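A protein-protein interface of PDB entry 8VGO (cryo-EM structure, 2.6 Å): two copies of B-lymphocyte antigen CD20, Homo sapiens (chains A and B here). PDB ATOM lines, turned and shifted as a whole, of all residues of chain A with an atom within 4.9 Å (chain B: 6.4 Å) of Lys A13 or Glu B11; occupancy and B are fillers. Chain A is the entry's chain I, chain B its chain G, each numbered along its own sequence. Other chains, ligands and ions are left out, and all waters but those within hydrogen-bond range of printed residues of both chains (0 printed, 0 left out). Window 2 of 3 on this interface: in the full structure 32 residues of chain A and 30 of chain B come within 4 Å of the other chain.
Glu A11 touches Lys B13, and with the chains exchanged Lys A13 touches Glu B11.
Lys A13 touches Thr B14, and with the chains exchanged Thr A14 touches Lys B13.
Thr A14 touches Ala B17, and with the chains exchanged Ala A17 touches Thr B14.
8 positions are printed for both chains.
Of the 6 pairs that touch across the chains among the printed residues, 6 have their exchanged pair printed and touching as well.
Among the printed residues, pairs that only touch across the chains: Lys A13 with Thr B14, Thr A14 with Lys B13, Thr A14 with Ala B17 and Ala A17 with Thr B14.
Of the 9 printed residues of chain B, 4 touch a printed residue of chain A.
Hydrophobic or aromatic side chains of chain B within 4 Å of the printed part of chain A: Ala B17.
Printed residues of chain A that touch a printed residue of chain B: Glu A11, Lys A13, Thr A14 and Ala A17.
Hydrophobic or aromatic side chains of chain A within 4 Å of the printed part of chain B: Ala A17.
Along chain A the printed residues that touch a printed residue of chain B span positions 11 to 17.
Among the printed residues, Asp or Glu carboxylates within 4 Å of a Lys or Arg side-chain nitrogen of the other chain: Glu A11 with Lys B13 and Lys A13 with Glu B11.
OE1 of Glu B11 is in salt-bridge range of NZ of Lys A13 (2.8 Å).
OE1 of Glu A11 lies within salt-bridge range of NZ of Lys B13, 2.8 Å away.
Of the printed residues of chain B, Lys A13 touches Glu B11 (2.8 Å) and Thr B14 (3.5 Å).
Of chain A, only Lys A13 comes within 4 Å of Glu B11.
Of the printed residues of chain A, Ala B17 touches Thr A14.
Of the printed residues of chain B, Glu A11 touches Lys B13 (2.8 Å).
Arg B10 touches none of the printed residues of chain A.
The nearest residue of chain B that does not touch Lys A13 is Lys B13 (5.6 Å).
The side-chain carboxylate of Glu B11 sits at hydrogen-bond distance from the side-chain hydroxyl of Thr B14, 2.7 Å away.
OG1 of Thr A14 lies within hydrogen-bond range of OE1 of Glu A11.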
ATOM      1  N   ARG A  10     -22.645 -11.843 -20.326  1.00  0.00           N
ATOM      2  CA  ARG A  10     -22.022 -11.679 -21.636  1.00  0.00           C
ATOM      3  C   ARG A  10     -20.584 -11.183 -21.530  1.00  0.00           C
ATOM      4  O   ARG A  10     -19.746 -11.532 -22.371  1.00  0.00           O
ATOM      5  CB  ARG A  10     -22.856 -10.718 -22.485  1.00  0.00           C
ATOM      6  CG  ARG A  10     -22.303 -10.463 -23.875  1.00  0.00           C
ATOM      7  CD  ARG A  10     -23.278  -9.659 -24.717  1.00  0.00           C
ATOM      8  NE  ARG A  10     -22.717  -9.305 -26.014  1.00  0.00           N
ATOM      9  CZ  ARG A  10     -23.429  -8.875 -27.047  1.00  0.00           C
ATOM     10  NH1 ARG A  10     -24.743  -8.742 -26.973  1.00  0.00           N
ATOM     11  NH2 ARG A  10     -22.806  -8.573 -28.183  1.00  0.00           N
ATOM     12  N   GLU A  11     -20.273 -10.384 -20.510  1.00  0.00           N
ATOM     13  CA  GLU A  11     -18.917  -9.901 -20.262  1.00  0.00           C
ATOM     14  C   GLU A  11     -17.909 -10.998 -19.926  1.00  0.00           C
ATOM     15  O   GLU A  11     -16.866 -10.712 -19.331  1.00  0.00           O
ATOM     16  CB  GLU A  11     -18.937  -8.876 -19.126  1.00  0.00           C
ATOM     17  CG  GLU A  11     -19.559  -7.539 -19.494  1.00  0.00           C
ATOM     18  CD  GLU A  11     -18.749  -6.780 -20.521  1.00  0.00           C
ATOM     19  OE1 GLU A  11     -17.522  -6.649 -20.331  1.00  0.00           O
ATOM     20  OE2 GLU A  11     -19.339  -6.311 -21.517  1.00  0.00           O
ATOM     21  N   SER A  12     -18.205 -12.251 -20.285  1.00  0.00           N
ATOM     22  CA  SER A  12     -17.408 -13.381 -19.815  1.00  0.00           C
ATOM     23  C   SER A  12     -15.955 -13.324 -20.276  1.00  0.00           C
ATOM     24  O   SER A  12     -15.089 -13.924 -19.631  1.00  0.00           O
ATOM     25  CB  SER A  12     -18.041 -14.692 -20.276  1.00  0.00           C
ATOM     26  OG  SER A  12     -19.237 -14.955 -19.564  1.00  0.00           O
ATOM     27  N   LYS A  13     -15.666 -12.615 -21.368  1.00  0.00           N
ATOM     28  CA  LYS A  13     -14.280 -12.311 -21.714  1.00  0.00           C
ATOM     29  C   LYS A  13     -13.633 -11.397 -20.679  1.00  0.00           C
ATOM     30  O   LYS A  13     -12.562 -11.704 -20.144  1.00  0.00           O
ATOM     31  CB  LYS A  13     -14.229 -11.670 -23.102  1.00  0.00           C
ATOM     32  CG  LYS A  13     -14.532 -12.627 -24.243  1.00  0.00           C
ATOM     33  CD  LYS A  13     -13.456 -13.685 -24.383  1.00  0.00           C
ATOM     34  CE  LYS A  13     -12.110 -13.045 -24.661  1.00  0.00           C
ATOM     35  NZ  LYS A  13     -12.086 -12.405 -26.003  1.00  0.00           N
ATOM     36  N   THR A  14     -14.274 -10.264 -20.392  1.00  0.00           N
ATOM     37  CA  THR A  14     -13.814  -9.360 -19.340  1.00  0.00           C
ATOM     38  C   THR A  14     -13.737 -10.047 -17.980  1.00  0.00           C
ATOM     39  O   THR A  14     -12.844  -9.751 -17.178  1.00  0.00           O
ATOM     40  CB  THR A  14     -14.731  -8.140 -19.264  1.00  0.00           C
ATOM     41  OG1 THR A  14     -15.043  -7.694 -20.589  1.00  0.00           O
ATOM     42  CG2 THR A  14     -14.052  -7.013 -18.510  1.00  0.00           C
ATOM     43  N   LEU A  15     -14.665 -10.960 -17.698  1.00  0.00           N
ATOM     44  CA  LEU A  15     -14.652 -11.679 -16.428  1.00  0.00           C
ATOM     45  C   LEU A  15     -13.583 -12.765 -16.362  1.00  0.00           C
ATOM     46  O   LEU A  15     -13.006 -12.997 -15.294  1.00  0.00           O
ATOM     47  CB  LEU A  15     -16.028 -12.290 -16.172  1.00  0.00           C
ATOM     48  CG  LEU A  15     -17.177 -11.294 -16.021  1.00  0.00           C
ATOM     49  CD1 LEU A  15     -18.487 -12.035 -15.833  1.00  0.00           C
ATOM     50  CD2 LEU A  15     -16.915 -10.344 -14.865  1.00  0.00           C
ATOM     51  N   GLY A  16     -13.309 -13.453 -17.469  1.00  0.00           N
ATOM     52  CA  GLY A  16     -12.260 -14.461 -17.452  1.00  0.00           C
ATOM     53  C   GLY A  16     -10.873 -13.906 -17.190  1.00  0.00           C
ATOM     54  O   GLY A  16     -10.044 -14.568 -16.562  1.00  0.00           O
ATOM     55  N   ALA A  17     -10.598 -12.693 -17.669  1.00  0.00           N
ATOM     56  CA  ALA A  17      -9.370 -11.993 -17.301  1.00  0.00           C
ATOM     57  C   ALA A  17      -9.297 -11.725 -15.801  1.00  0.00           C
ATOM     58  O   ALA A  17      -8.258 -11.941 -15.170  1.00  0.00           O
ATOM     59  CB  ALA A  17      -9.265 -10.685 -18.085  1.00  0.00           C
ATOM     60  N   LEU A  64     -12.509 -18.213 -21.151  1.00  0.00           N
ATOM     61  CA  LEU A  64     -12.096 -17.288 -22.202  1.00  0.00           C
ATOM     62  C   LEU A  64     -12.134 -17.932 -23.581  1.00  0.00           C
ATOM     63  O   LEU A  64     -12.392 -17.247 -24.578  1.00  0.00           O
ATOM     64  CB  LEU A  64     -10.698 -16.749 -21.915  1.00  0.00           C
ATOM     65  CG  LEU A  64     -10.587 -15.805 -20.723  1.00  0.00           C
ATOM     66  CD1 LEU A  64      -9.154 -15.349 -20.547  1.00  0.00           C
ATOM     67  CD2 LEU A  64     -11.499 -14.618 -20.951  1.00  0.00           C
ATOM     68  N   MET B   9      -5.161  -3.675 -29.442  1.00  0.00           N
ATOM     69  CA  MET B   9      -5.604  -4.987 -29.895  1.00  0.00           C
ATOM     70  C   MET B   9      -7.122  -5.086 -29.721  1.00  0.00           C
ATOM     71  O   MET B   9      -7.711  -4.338 -28.941  1.00  0.00           O
ATOM     72  CB  MET B   9      -4.861  -6.093 -29.127  1.00  0.00           C
ATOM     73  CG  MET B   9      -5.321  -7.519 -29.405  1.00  0.00           C
ATOM     74  SD  MET B   9      -4.113  -8.770 -28.919  1.00  0.00           S
ATOM     75  CE  MET B   9      -3.960  -8.454 -27.164  1.00  0.00           C
ATOM     76  N   ARG B  10      -7.750  -6.000 -30.465  1.00  0.00           N
ATOM     77  CA  ARG B  10      -9.197  -6.181 -30.373  1.00  0.00           C
ATOM     78  C   ARG B  10      -9.629  -6.662 -28.992  1.00  0.00           C
ATOM     79  O   ARG B  10     -10.726  -6.320 -28.534  1.00  0.00           O
ATOM     80  CB  ARG B  10      -9.661  -7.164 -31.450  1.00  0.00           C
ATOM     81  CG  ARG B  10     -11.154  -7.437 -31.452  1.00  0.00           C
ATOM     82  CD  ARG B  10     -11.559  -8.266 -32.659  1.00  0.00           C
ATOM     83  NE  ARG B  10     -12.968  -8.637 -32.618  1.00  0.00           N
ATOM     84  CZ  ARG B  10     -13.653  -9.092 -33.657  1.00  0.00           C
ATOM     85  NH1 ARG B  10     -13.091  -9.234 -34.847  1.00  0.00           N
ATOM     86  NH2 ARG B  10     -14.935  -9.409 -33.501  1.00  0.00           N
ATOM     87  N   GLU B  11      -8.789  -7.440 -28.312  1.00  0.00           N
ATOM     88  CA  GLU B  11      -9.060  -7.907 -26.954  1.00  0.00           C
ATOM     89  C   GLU B  11      -9.136  -6.794 -25.911  1.00  0.00           C
ATOM     90  O   GLU B  11      -8.969  -7.061 -24.716  1.00  0.00           O
ATOM     91  CB  GLU B  11      -7.986  -8.914 -26.535  1.00  0.00           C
ATOM     92  CG  GLU B  11      -8.079 -10.263 -27.229  1.00  0.00           C
ATOM     93  CD  GLU B  11      -9.326 -11.030 -26.849  1.00  0.00           C
ATOM     94  OE1 GLU B  11      -9.607 -11.147 -25.638  1.00  0.00           O
ATOM     95  OE2 GLU B  11     -10.025 -11.521 -27.760  1.00  0.00           O
ATOM     96  N   SER B  12      -9.374  -5.551 -26.337  1.00  0.00           N
ATOM     97  CA  SER B  12      -9.248  -4.406 -25.438  1.00  0.00           C
ATOM     98  C   SER B  12     -10.217  -4.458 -24.261  1.00  0.00           C
ATOM     99  O   SER B  12      -9.948  -3.840 -23.226  1.00  0.00           O
ATOM    100  CB  SER B  12      -9.455  -3.109 -26.217  1.00  0.00           C
ATOM    101  OG  SER B  12      -8.352  -2.845 -27.066  1.00  0.00           O
ATOM    102  N   LYS B  13     -11.330  -5.181 -24.390  1.00  0.00           N
ATOM    103  CA  LYS B  13     -12.165  -5.477 -23.228  1.00  0.00           C
ATOM    104  C   LYS B  13     -11.434  -6.368 -22.229  1.00  0.00           C
ATOM    105  O   LYS B  13     -11.340  -6.043 -21.040  1.00  0.00           O
ATOM    106  CB  LYS B  13     -13.463  -6.141 -23.689  1.00  0.00           C
ATOM    107  CG  LYS B  13     -14.421  -5.205 -24.409  1.00  0.00           C
ATOM    108  CD  LYS B  13     -14.963  -4.140 -23.478  1.00  0.00           C
ATOM    109  CE  LYS B  13     -15.713  -4.772 -22.323  1.00  0.00           C
ATOM    110  NZ  LYS B  13     -16.961  -5.433 -22.791  1.00  0.00           N
ATOM    111  N   THR B  14     -10.915  -7.502 -22.701  1.00  0.00           N
ATOM    112  CA  THR B  14     -10.098  -8.384 -21.869  1.00  0.00           C
ATOM    113  C   THR B  14      -8.874  -7.675 -21.302  1.00  0.00           C
ATOM    114  O   THR B  14      -8.460  -7.948 -20.169  1.00  0.00           O
ATOM    115  CB  THR B  14      -9.672  -9.612 -22.675  1.00  0.00           C
ATOM    116  OG1 THR B  14     -10.778 -10.082 -23.453  1.00  0.00           O
ATOM    117  CG2 THR B  14      -9.212 -10.720 -21.747  1.00  0.00           C
ATOM    118  N   LEU B  15      -8.276  -6.768 -22.072  1.00  0.00           N
ATOM    119  CA  LEU B  15      -7.110  -6.028 -21.600  1.00  0.00           C
ATOM    120  C   LEU B  15      -7.459  -4.937 -20.594  1.00  0.00           C
ATOM    121  O   LEU B  15      -6.687  -4.693 -19.661  1.00  0.00           O
ATOM    122  CB  LEU B  15      -6.373  -5.420 -22.791  1.00  0.00           C
ATOM    123  CG  LEU B  15      -5.797  -6.419 -23.794  1.00  0.00           C
ATOM    124  CD1 LEU B  15      -5.146  -5.681 -24.948  1.00  0.00           C
ATOM    125  CD2 LEU B  15      -4.811  -7.353 -23.116  1.00  0.00           C
ATOM    126  N   GLY B  16      -8.591  -4.257 -20.762  1.00  0.00           N
ATOM    127  CA  GLY B  16      -8.973  -3.243 -19.792  1.00  0.00           C
ATOM    128  C   GLY B  16      -9.242  -3.791 -18.402  1.00  0.00           C
ATOM    129  O   GLY B  16      -8.981  -3.115 -17.404  1.00  0.00           O
ATOM    130  N   ALA B  17      -9.772  -5.011 -18.317  1.00  0.00           N
ATOM    131  CA  ALA B  17      -9.887  -5.699 -17.034  1.00  0.00           C
ATOM    132  C   ALA B  17      -8.523  -5.940 -16.396  1.00  0.00           C
ATOM    133  O   ALA B  17      -8.337  -5.713 -15.195  1.00  0.00           O
ATOM    134  CB  ALA B  17     -10.632  -7.020 -17.219  1.00  0.00           C
